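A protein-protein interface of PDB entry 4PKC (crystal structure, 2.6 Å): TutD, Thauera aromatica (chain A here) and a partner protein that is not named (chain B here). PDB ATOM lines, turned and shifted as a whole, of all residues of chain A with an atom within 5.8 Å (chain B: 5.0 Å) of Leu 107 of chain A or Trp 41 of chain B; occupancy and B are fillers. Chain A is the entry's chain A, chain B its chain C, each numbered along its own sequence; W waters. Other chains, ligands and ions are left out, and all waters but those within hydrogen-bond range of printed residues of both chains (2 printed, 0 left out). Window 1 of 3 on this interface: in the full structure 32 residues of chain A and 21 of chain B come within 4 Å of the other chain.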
ATOM      1  N   LEU A 102     -16.454 -11.138 -17.157  1.00  0.00           N
ATOM      2  CA  LEU A 102     -17.251 -10.149 -16.434  1.00  0.00           C
ATOM      3  C   LEU A 102     -16.482  -8.862 -16.152  1.00  0.00           C
ATOM      4  O   LEU A 102     -17.028  -7.764 -16.270  1.00  0.00           O
ATOM      5  CB  LEU A 102     -17.761 -10.736 -15.116  1.00  0.00           C
ATOM      6  CG  LEU A 102     -18.758 -11.891 -15.211  1.00  0.00           C
ATOM      7  CD1 LEU A 102     -19.184 -12.341 -13.822  1.00  0.00           C
ATOM      8  CD2 LEU A 102     -19.966 -11.492 -16.041  1.00  0.00           C
ATOM      9  N   SER A 105     -15.660  -6.972 -19.736  1.00  0.00           N
ATOM     10  CA  SER A 105     -16.733  -6.798 -20.712  1.00  0.00           C
ATOM     11  C   SER A 105     -17.292  -5.382 -20.747  1.00  0.00           C
ATOM     12  O   SER A 105     -17.482  -4.745 -19.710  1.00  0.00           O
ATOM     13  CB  SER A 105     -17.875  -7.776 -20.437  1.00  0.00           C
ATOM     14  OG  SER A 105     -17.629  -9.028 -21.050  1.00  0.00           O
ATOM     15  N   THR A 106     -17.556  -4.901 -21.958  1.00  0.00           N
ATOM     16  CA  THR A 106     -18.267  -3.645 -22.143  1.00  0.00           C
ATOM     17  C   THR A 106     -19.707  -3.810 -21.674  1.00  0.00           C
ATOM     18  O   THR A 106     -20.395  -4.744 -22.088  1.00  0.00           O
ATOM     19  CB  THR A 106     -18.253  -3.192 -23.617  1.00  0.00           C
ATOM     20  OG1 THR A 106     -16.899  -3.046 -24.065  1.00  0.00           O
ATOM     21  CG2 THR A 106     -18.988  -1.868 -23.777  1.00  0.00           C
ATOM     22  N   LEU A 107     -20.156  -2.911 -20.804  1.00  0.00           N
ATOM     23  CA  LEU A 107     -21.510  -2.981 -20.265  1.00  0.00           C
ATOM     24  C   LEU A 107     -22.447  -2.054 -21.031  1.00  0.00           C
ATOM     25  O   LEU A 107     -22.019  -1.031 -21.562  1.00  0.00           O
ATOM     26  CB  LEU A 107     -21.512  -2.634 -18.775  1.00  0.00           C
ATOM     27  CG  LEU A 107     -20.593  -3.507 -17.916  1.00  0.00           C
ATOM     28  CD1 LEU A 107     -20.657  -3.095 -16.458  1.00  0.00           C
ATOM     29  CD2 LEU A 107     -20.940  -4.981 -18.077  1.00  0.00           C
ATOM     30  N   VAL A 108     -23.724  -2.419 -21.088  1.00  0.00           N
ATOM     31  CA  VAL A 108     -24.694  -1.686 -21.894  1.00  0.00           C
ATOM     32  C   VAL A 108     -25.854  -1.139 -21.065  1.00  0.00           C
ATOM     33  O   VAL A 108     -26.466  -1.860 -20.275  1.00  0.00           O
ATOM     34  CB  VAL A 108     -25.268  -2.574 -23.018  1.00  0.00           C
ATOM     35  CG1 VAL A 108     -26.244  -1.784 -23.882  1.00  0.00           C
ATOM     36  CG2 VAL A 108     -24.146  -3.151 -23.866  1.00  0.00           C
ATOM     37  N   LEU A 109     -26.145   0.144 -21.251  1.00  0.00           N
ATOM     38  CA  LEU A 109     -27.311   0.776 -20.646  1.00  0.00           C
ATOM     39  C   LEU A 109     -28.108   1.509 -21.715  1.00  0.00           C
ATOM     40  O   LEU A 109     -27.573   2.369 -22.411  1.00  0.00           O
ATOM     41  CB  LEU A 109     -26.895   1.747 -19.541  1.00  0.00           C
ATOM     42  CG  LEU A 109     -27.997   2.657 -18.990  1.00  0.00           C
ATOM     43  CD1 LEU A 109     -29.077   1.844 -18.295  1.00  0.00           C
ATOM     44  CD2 LEU A 109     -27.414   3.701 -18.050  1.00  0.00           C
ATOM     45  N   GLN A 110     -29.386   1.169 -21.847  1.00  0.00           N
ATOM     46  CA  GLN A 110     -30.236   1.798 -22.851  1.00  0.00           C
ATOM     47  C   GLN A 110     -31.239   2.753 -22.217  1.00  0.00           C
ATOM     48  O   GLN A 110     -31.432   2.751 -21.002  1.00  0.00           O
ATOM     49  CB  GLN A 110     -30.973   0.739 -23.671  1.00  0.00           C
ATOM     50  CG  GLN A 110     -30.062  -0.262 -24.357  1.00  0.00           C
ATOM     51  CD  GLN A 110     -30.817  -1.183 -25.292  1.00  0.00           C
ATOM     52  OE1 GLN A 110     -31.454  -0.731 -26.244  1.00  0.00           O
ATOM     53  NE2 GLN A 110     -30.759  -2.482 -25.019  1.00  0.00           N
ATOM     54  N   GLU A 111     -31.873   3.570 -23.051  1.00  0.00           N
ATOM     55  CA  GLU A 111     -32.887   4.508 -22.588  1.00  0.00           C
ATOM     56  C   GLU A 111     -34.172   3.778 -22.212  1.00  0.00           C
ATOM     57  O   GLU A 111     -34.432   2.679 -22.703  1.00  0.00           O
ATOM     58  CB  GLU A 111     -33.169   5.563 -23.660  1.00  0.00           C
ATOM     59  CG  GLU A 111     -33.543   4.986 -25.017  1.00  0.00           C
ATOM     60  CD  GLU A 111     -33.932   6.058 -26.015  1.00  0.00           C
ATOM     61  OE1 GLU A 111     -34.564   7.052 -25.601  1.00  0.00           O
ATOM     62  OE2 GLU A 111     -33.600   5.911 -27.211  1.00  0.00           O
ATOM     63  N   TYR A 118     -26.758  -6.726 -19.928  1.00  0.00           N
ATOM     64  CA  TYR A 118     -26.676  -7.437 -21.197  1.00  0.00           C
ATOM     65  C   TYR A 118     -25.530  -8.446 -21.183  1.00  0.00           C
ATOM     66  O   TYR A 118     -24.684  -8.432 -20.288  1.00  0.00           O
ATOM     67  CB  TYR A 118     -26.514  -6.454 -22.360  1.00  0.00           C
ATOM     68  CG  TYR A 118     -26.998  -7.013 -23.679  1.00  0.00           C
ATOM     69  CD1 TYR A 118     -28.332  -7.358 -23.858  1.00  0.00           C
ATOM     70  CD2 TYR A 118     -26.124  -7.202 -24.741  1.00  0.00           C
ATOM     71  CE1 TYR A 118     -28.783  -7.876 -25.056  1.00  0.00           C
ATOM     72  CE2 TYR A 118     -26.567  -7.718 -25.947  1.00  0.00           C
ATOM     73  CZ  TYR A 118     -27.897  -8.053 -26.097  1.00  0.00           C
ATOM     74  OH  TYR A 118     -28.343  -8.567 -27.293  1.00  0.00           O
ATOM     75  N   ALA A 120     -23.429  -9.088 -23.927  1.00  0.00           N
ATOM     76  CA  ALA A 120     -22.461  -8.821 -24.987  1.00  0.00           C
ATOM     77  C   ALA A 120     -21.966  -7.378 -24.910  1.00  0.00           C
ATOM     78  O   ALA A 120     -22.431  -6.601 -24.076  1.00  0.00           O
ATOM     79  CB  ALA A 120     -23.071  -9.106 -26.355  1.00  0.00           C
ATOM     80  N   GLU A 121     -21.024  -7.025 -25.780  1.00  0.00           N
ATOM     81  CA  GLU A 121     -20.436  -5.686 -25.777  1.00  0.00           C
ATOM     82  C   GLU A 121     -21.304  -4.682 -26.527  1.00  0.00           C
ATOM     83  O   GLU A 121     -21.069  -3.474 -26.468  1.00  0.00           O
ATOM     84  CB  GLU A 121     -19.037  -5.711 -26.394  1.00  0.00           C
ATOM     85  CG  GLU A 121     -18.994  -6.130 -27.858  1.00  0.00           C
ATOM     86  CD  GLU A 121     -18.835  -7.630 -28.042  1.00  0.00           C
ATOM     87  OE1 GLU A 121     -19.552  -8.396 -27.366  1.00  0.00           O
ATOM     88  OE2 GLU A 121     -17.986  -8.040 -28.862  1.00  0.00           O
ATOM     89  N   TRP A 262     -19.356  -7.147 -11.303  1.00  0.00           N
ATOM     90  CA  TRP A 262     -19.949  -6.933 -12.618  1.00  0.00           C
ATOM     91  C   TRP A 262     -21.288  -6.206 -12.517  1.00  0.00           C
ATOM     92  O   TRP A 262     -21.600  -5.341 -13.335  1.00  0.00           O
ATOM     93  CB  TRP A 262     -20.113  -8.279 -13.327  1.00  0.00           C
ATOM     94  CG  TRP A 262     -20.953  -8.269 -14.563  1.00  0.00           C
ATOM     95  CD1 TRP A 262     -20.625  -7.740 -15.775  1.00  0.00           C
ATOM     96  CD2 TRP A 262     -22.250  -8.860 -14.719  1.00  0.00           C
ATOM     97  NE1 TRP A 262     -21.645  -7.947 -16.672  1.00  0.00           N
ATOM     98  CE2 TRP A 262     -22.652  -8.633 -16.049  1.00  0.00           C
ATOM     99  CE3 TRP A 262     -23.112  -9.550 -13.860  1.00  0.00           C
ATOM    100  CZ2 TRP A 262     -23.881  -9.072 -16.541  1.00  0.00           C
ATOM    101  CZ3 TRP A 262     -24.330  -9.983 -14.351  1.00  0.00           C
ATOM    102  CH2 TRP A 262     -24.703  -9.743 -15.679  1.00  0.00           C
ATOM    103  N   ARG A 265     -20.529  -2.605 -11.330  1.00  0.00           N
ATOM    104  CA  ARG A 265     -19.969  -1.810 -12.415  1.00  0.00           C
ATOM    105  C   ARG A 265     -21.087  -1.415 -13.374  1.00  0.00           C
ATOM    106  O   ARG A 265     -21.026  -0.371 -14.021  1.00  0.00           O
ATOM    107  CB  ARG A 265     -18.862  -2.575 -13.146  1.00  0.00           C
ATOM    108  CG  ARG A 265     -18.142  -1.753 -14.209  1.00  0.00           C
ATOM    109  CD  ARG A 265     -16.808  -2.373 -14.598  1.00  0.00           C
ATOM    110  NE  ARG A 265     -16.951  -3.731 -15.110  1.00  0.00           N
ATOM    111  CZ  ARG A 265     -17.164  -4.028 -16.387  1.00  0.00           C
ATOM    112  NH1 ARG A 265     -17.281  -5.293 -16.767  1.00  0.00           N
ATOM    113  NH2 ARG A 265     -17.261  -3.059 -17.286  1.00  0.00           N
ATOM    114  N   GLN A 266     -22.111  -2.260 -13.452  1.00  0.00           N
ATOM    115  CA  GLN A 266     -23.305  -1.955 -14.231  1.00  0.00           C
ATOM    116  C   GLN A 266     -24.052  -0.790 -13.596  1.00  0.00           C
ATOM    117  O   GLN A 266     -24.582   0.077 -14.291  1.00  0.00           O
ATOM    118  CB  GLN A 266     -24.216  -3.179 -14.330  1.00  0.00           C
ATOM    119  CG  GLN A 266     -25.533  -2.922 -15.049  1.00  0.00           C
ATOM    120  CD  GLN A 266     -25.378  -2.870 -16.557  1.00  0.00           C
ATOM    121  OE1 GLN A 266     -24.795  -3.770 -17.162  1.00  0.00           O
ATOM    122  NE2 GLN A 266     -25.897  -1.814 -17.171  1.00  0.00           N
ATOM    123  N   LEU A 269     -22.329   2.550 -14.165  1.00  0.00           N
ATOM    124  CA  LEU A 269     -22.666   3.077 -15.482  1.00  0.00           C
ATOM    125  C   LEU A 269     -23.935   3.920 -15.420  1.00  0.00           C
ATOM    126  O   LEU A 269     -24.014   4.984 -16.035  1.00  0.00           O
ATOM    127  CB  LEU A 269     -22.838   1.939 -16.489  1.00  0.00           C
ATOM    128  CG  LEU A 269     -23.373   2.315 -17.874  1.00  0.00           C
ATOM    129  CD1 LEU A 269     -22.493   3.366 -18.530  1.00  0.00           C
ATOM    130  CD2 LEU A 269     -23.477   1.080 -18.753  1.00  0.00           C
ATOM    131  N   VAL A 273     -24.086   7.952 -16.305  1.00  0.00           N
ATOM    132  CA  VAL A 273     -24.999   8.461 -17.323  1.00  0.00           C
ATOM    133  C   VAL A 273     -25.986   9.470 -16.731  1.00  0.00           C
ATOM    134  O   VAL A 273     -26.308  10.483 -17.355  1.00  0.00           O
ATOM    135  CB  VAL A 273     -25.772   7.308 -18.002  1.00  0.00           C
ATOM    136  CG1 VAL A 273     -26.902   7.842 -18.870  1.00  0.00           C
ATOM    137  CG2 VAL A 273     -24.822   6.456 -18.826  1.00  0.00           C
ATOM    138  N   PHE A 277     -24.645  12.435 -18.721  1.00  0.00           N
ATOM    139  CA  PHE A 277     -25.205  12.222 -20.053  1.00  0.00           C
ATOM    140  C   PHE A 277     -26.710  12.482 -20.136  1.00  0.00           C
ATOM    141  O   PHE A 277     -27.177  13.142 -21.062  1.00  0.00           O
ATOM    142  CB  PHE A 277     -24.904  10.796 -20.525  1.00  0.00           C
ATOM    143  CG  PHE A 277     -23.445  10.537 -20.786  1.00  0.00           C
ATOM    144  CD1 PHE A 277     -22.583  10.226 -19.746  1.00  0.00           C
ATOM    145  CD2 PHE A 277     -22.938  10.596 -22.074  1.00  0.00           C
ATOM    146  CE1 PHE A 277     -21.243   9.986 -19.983  1.00  0.00           C
ATOM    147  CE2 PHE A 277     -21.597  10.355 -22.319  1.00  0.00           C
ATOM    148  CZ  PHE A 277     -20.749  10.049 -21.271  1.00  0.00           C
ATOM    149  N   GLU A 278     -27.464  11.956 -19.175  1.00  0.00           N
ATOM    150  CA  GLU A 278     -28.918  12.097 -19.193  1.00  0.00           C
ATOM    151  C   GLU A 278     -29.346  13.533 -18.897  1.00  0.00           C
ATOM    152  O   GLU A 278     -28.837  14.161 -17.969  1.00  0.00           O
ATOM    153  CB  GLU A 278     -29.561  11.139 -18.190  1.00  0.00           C
ATOM    154  CG  GLU A 278     -31.081  11.177 -18.197  1.00  0.00           C
ATOM    155  CD  GLU A 278     -31.664  10.867 -19.561  1.00  0.00           C
ATOM    156  OE1 GLU A 278     -32.612  11.565 -19.977  1.00  0.00           O
ATOM    157  OE2 GLU A 278     -31.174   9.924 -20.220  1.00  0.00           O
ATOM    158  N   LEU A 287     -32.382   6.450 -12.898  1.00  0.00           N
ATOM    159  CA  LEU A 287     -31.095   5.784 -13.071  1.00  0.00           C
ATOM    160  C   LEU A 287     -30.339   5.682 -11.751  1.00  0.00           C
ATOM    161  O   LEU A 287     -29.555   4.755 -11.546  1.00  0.00           O
ATOM    162  CB  LEU A 287     -30.243   6.523 -14.104  1.00  0.00           C
ATOM    163  CG  LEU A 287     -30.699   6.432 -15.560  1.00  0.00           C
ATOM    164  CD1 LEU A 287     -29.793   7.264 -16.452  1.00  0.00           C
ATOM    165  CD2 LEU A 287     -30.724   4.983 -16.016  1.00  0.00           C
ATOM    166  N   VAL B  30     -16.867   5.624 -20.967  1.00  0.00           N
ATOM    167  CA  VAL B  30     -18.283   5.716 -21.297  1.00  0.00           C
ATOM    168  C   VAL B  30     -18.503   6.500 -22.585  1.00  0.00           C
ATOM    169  O   VAL B  30     -18.137   7.669 -22.682  1.00  0.00           O
ATOM    170  CB  VAL B  30     -19.085   6.375 -20.161  1.00  0.00           C
ATOM    171  CG1 VAL B  30     -20.562   6.425 -20.521  1.00  0.00           C
ATOM    172  CG2 VAL B  30     -18.873   5.620 -18.858  1.00  0.00           C
ATOM    173  N   ARG B  31     -19.101   5.842 -23.574  1.00  0.00           N
ATOM    174  CA  ARG B  31     -19.398   6.479 -24.850  1.00  0.00           C
ATOM    175  C   ARG B  31     -20.884   6.371 -25.170  1.00  0.00           C
ATOM    176  O   ARG B  31     -21.473   5.295 -25.071  1.00  0.00           O
ATOM    177  CB  ARG B  31     -18.570   5.850 -25.974  1.00  0.00           C
ATOM    178  CG  ARG B  31     -17.088   5.736 -25.661  1.00  0.00           C
ATOM    179  CD  ARG B  31     -16.288   5.265 -26.868  1.00  0.00           C
ATOM    180  NE  ARG B  31     -16.302   6.245 -27.950  1.00  0.00           N
ATOM    181  CZ  ARG B  31     -15.495   6.204 -29.006  1.00  0.00           C
ATOM    182  NH1 ARG B  31     -15.579   7.139 -29.944  1.00  0.00           N
ATOM    183  NH2 ARG B  31     -14.601   5.232 -29.125  1.00  0.00           N
ATOM    184  N   GLU B  32     -21.492   7.490 -25.550  1.00  0.00           N
ATOM    185  CA  GLU B  32     -22.899   7.494 -25.927  1.00  0.00           C
ATOM    186  C   GLU B  32     -23.059   7.219 -27.418  1.00  0.00           C
ATOM    187  O   GLU B  32     -22.393   7.839 -28.246  1.00  0.00           O
ATOM    188  CB  GLU B  32     -23.554   8.826 -25.562  1.00  0.00           C
ATOM    189  CG  GLU B  32     -25.005   8.938 -25.998  1.00  0.00           C
ATOM    190  CD  GLU B  32     -25.642  10.249 -25.585  1.00  0.00           C
ATOM    191  OE1 GLU B  32     -26.309  10.880 -26.433  1.00  0.00           O
ATOM    192  OE2 GLU B  32     -25.481  10.647 -24.411  1.00  0.00           O
ATOM    193  N   LYS B  33     -23.937   6.280 -27.752  1.00  0.00           N
ATOM    194  CA  LYS B  33     -24.214   5.950 -29.145  1.00  0.00           C
ATOM    195  C   LYS B  33     -25.716   5.958 -29.403  1.00  0.00           C
ATOM    196  O   LYS B  33     -26.513   5.942 -28.465  1.00  0.00           O
ATOM    197  CB  LYS B  33     -23.622   4.586 -29.510  1.00  0.00           C
ATOM    198  CG  LYS B  33     -22.144   4.436 -29.181  1.00  0.00           C
ATOM    199  CD  LYS B  33     -21.596   3.105 -29.671  1.00  0.00           C
ATOM    200  CE  LYS B  33     -21.394   3.104 -31.176  1.00  0.00           C
ATOM    201  NZ  LYS B  33     -20.329   4.060 -31.583  1.00  0.00           N
ATOM    202  N   LYS B  39     -31.201   5.357 -28.166  1.00  0.00           N
ATOM    203  CA  LYS B  39     -29.934   5.745 -27.558  1.00  0.00           C
ATOM    204  C   LYS B  39     -29.496   4.754 -26.484  1.00  0.00           C
ATOM    205  O   LYS B  39     -30.325   4.199 -25.762  1.00  0.00           O
ATOM    206  CB  LYS B  39     -30.048   7.150 -26.964  1.00  0.00           C
ATOM    207  CG  LYS B  39     -28.764   7.687 -26.356  1.00  0.00           C
ATOM    208  CD  LYS B  39     -28.986   9.052 -25.728  1.00  0.00           C
ATOM    209  CE  LYS B  39     -29.499  10.054 -26.749  1.00  0.00           C
ATOM    210  NZ  LYS B  39     -29.752  11.382 -26.128  1.00  0.00           N
ATOM    211  N   TYR B  40     -28.189   4.530 -26.384  1.00  0.00           N
ATOM    212  CA  TYR B  40     -27.638   3.685 -25.331  1.00  0.00           C
ATOM    213  C   TYR B  40     -26.212   4.098 -24.979  1.00  0.00           C
ATOM    214  O   TYR B  40     -25.598   4.906 -25.674  1.00  0.00           O
ATOM    215  CB  TYR B  40     -27.679   2.211 -25.742  1.00  0.00           C
ATOM    216  CG  TYR B  40     -26.866   1.874 -26.971  1.00  0.00           C
ATOM    217  CD1 TYR B  40     -27.407   2.007 -28.242  1.00  0.00           C
ATOM    218  CD2 TYR B  40     -25.562   1.406 -26.860  1.00  0.00           C
ATOM    219  CE1 TYR B  40     -26.671   1.693 -29.370  1.00  0.00           C
ATOM    220  CE2 TYR B  40     -24.816   1.089 -27.981  1.00  0.00           C
ATOM    221  CZ  TYR B  40     -25.377   1.235 -29.234  1.00  0.00           C
ATOM    222  OH  TYR B  40     -24.642   0.922 -30.353  1.00  0.00           O
ATOM    223  N   TRP B  41     -25.691   3.537 -23.891  1.00  0.00           N
ATOM    224  CA  TRP B  41     -24.354   3.877 -23.419  1.00  0.00           C
ATOM    225  C   TRP B  41     -23.493   2.633 -23.220  1.00  0.00           C
ATOM    226  O   TRP B  41     -23.992   1.576 -22.832  1.00  0.00           O
ATOM    227  CB  TRP B  41     -24.441   4.671 -22.114  1.00  0.00           C
ATOM    228  CG  TRP B  41     -25.122   5.995 -22.273  1.00  0.00           C
ATOM    229  CD1 TRP B  41     -24.526   7.199 -22.511  1.00  0.00           C
ATOM    230  CD2 TRP B  41     -26.530   6.252 -22.209  1.00  0.00           C
ATOM    231  NE1 TRP B  41     -25.473   8.190 -22.598  1.00  0.00           N
ATOM    232  CE2 TRP B  41     -26.713   7.635 -22.415  1.00  0.00           C
ATOM    233  CE3 TRP B  41     -27.654   5.450 -21.995  1.00  0.00           C
ATOM    234  CZ2 TRP B  41     -27.973   8.230 -22.415  1.00  0.00           C
ATOM    235  CZ3 TRP B  41     -28.904   6.041 -21.995  1.00  0.00           C
ATOM    236  CH2 TRP B  41     -29.053   7.418 -22.204  1.00  0.00           C
ATOM    237  N   LEU B  42     -22.197   2.769 -23.489  1.00  0.00           N
ATOM    238  CA  LEU B  42     -21.264   1.654 -23.376  1.00  0.00           C
ATOM    239  C   LEU B  42     -20.139   1.975 -22.398  1.00  0.00           C
ATOM    240  O   LEU B  42     -19.489   3.011 -22.511  1.00  0.00           O
ATOM    241  CB  LEU B  42     -20.682   1.301 -24.746  1.00  0.00           C
ATOM    242  CG  LEU B  42     -21.677   0.920 -25.843  1.00  0.00           C
ATOM    243  CD1 LEU B  42     -20.952   0.594 -27.139  1.00  0.00           C
ATOM    244  CD2 LEU B  42     -22.534  -0.252 -25.404  1.00  0.00           C
ATOM    245  N   SER B  43     -19.912   1.079 -21.441  1.00  0.00           N
ATOM    246  CA  SER B  43     -18.870   1.272 -20.435  1.00  0.00           C
ATOM    247  C   SER B  43     -17.773   0.216 -20.554  1.00  0.00           C
ATOM    248  O   SER B  43     -17.983  -0.951 -20.221  1.00  0.00           O
ATOM    249  CB  SER B  43     -19.473   1.242 -19.030  1.00  0.00           C
ATOM    250  OG  SER B  43     -18.470   1.394 -18.040  1.00  0.00           O
HETATM  251  O   HOH W   1     -31.652   2.265 -27.418  1.00  0.00           O
HETATM  252  O   HOH W   2     -16.565  -0.255 -17.489  1.00  0.00           O
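Of the 19 printed residues of chain A, 13 touch a printed residue of chain B. Printed residues of chain A that touch a printed residue of chain B: Ser 105, Thr 106, Leu 107, Val 108, Leu 109, Gln 110, Glu 111, Glu 121, Arg 265, Leu 269, Val 273, Phe 277 and Glu 278. Of the 9 printed residues of chain B, 7 touch a printed residue of chain A. Hydrophobic or aromatic side chains of chain B within 4 Å of the printed part of chain A: Val 30, Tyr 40, Trp 41 and Leu 42.
Water W2 lies within hydrogen-bond range of OG of Ser 43 of chain B and NH2 of Arg 265 of chain A. Water W1 bridges O of Lys 39 of chain B (2.9 Å) and OE1 of Gln 110 of chain A (3.2 Å).
NH1 of Arg 265 of chain A is in hydrogen-bond range of O of Leu 102 of chain A (2.5 Å). The side-chain amide nitrogen of Gln 266 of chain A lies within hydrogen-bond range of the backbone carbonyl oxygen of Val 108 of chain A, 3.2 Å away. N of Glu 278 of chain A sits at hydrogen-bond distance from O of Val 273 of chain A, at 2.6 Å. OE1 of Glu 32 of chain B is in salt-bridge range of NZ of Lys 39 of chain B, 3.5 Å away. OE2 of Glu 32 of chain B lies within hydrogen-bond range of NE1 of Trp 41 of chain B, at 3.1 Å. O of Tyr 40 of chain B lies within hydrogen-bond range of N of Lys 33 of chain B (3.0 Å).
Ser 105 of chain A touches Ser 43 of chain B (O to O, 3.9 Å). Leu 42 of chain B touches Thr 106 of chain A. O of Leu 107 of chain A touches O of Trp 41 of chain B, 3.5 Å away. Val 108 of chain A touches Trp 41 of chain B. Leu 109 of chain A touches Tyr 40 of chain B (O to CA, 3.2 Å). O of Glu 121 of chain A touches CD2 of Leu 42 of chain B (3.7 Å). NH2 of Arg 265 of chain A touches O of Ser 43 of chain B, 3.7 Å away. CB of Ser 43 of chain B touches CD1 of Leu 269 of chain A (3.7 Å). CG1 of Val 30 of chain B touches CE1 of Phe 277 of chain A (3.7 Å). Glu 32 of chain B touches Phe 277 of chain A.
Printed residues of chain B within 4 Å of Thr 106 of chain A: Leu 42 (3.7 Å) and Ser 43 (3.3 Å). Leu 107 of chain A touches three residues of chain B. Printed residues of chain B within 4 Å of Val 108 of chain A: Trp 41 (3.5 Å) and Leu 42 (3.7 Å). Printed residues of chain B within 4 Å of Glu 121 of chain A: Leu 42 (3.7 Å). Trp 262 of chain A touches none of the printed residues of chain B. Printed residues of chain B within 4 Å of Val 273 of chain A: Trp 41. Printed residues of chain B within 4 Å of Phe 277 of chain A: Val 30 (3.7 Å), Glu 32 (3.5 Å) and Trp 41 (3.4 Å). Of the printed residues of chain A, Trp 41 of chain B touches Leu 107, Val 108, Leu 109, Val 273, Phe 277 and Glu 278. The nearest printed residue of chain B that does not touch Leu 107 of chain A is Tyr 40 of chain B (6.8 Å).
The backbone NH (N) of Leu 107 of chain A lies within hydrogen-bond range of the backbone carbonyl oxygen (O) of Ser 43 of chain B (3.0 Å). The backbone NH (N) of Trp 41 of chain B sits at hydrogen-bond distance from the backbone carbonyl oxygen (O) of Leu 109 of chain A (2.7 Å). The side-chain carboxylate (OE2) of Glu 111 of chain A sits at hydrogen-bond distance from the backbone NH (N) of Lys 39 of chain B, 2.6 Å away.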
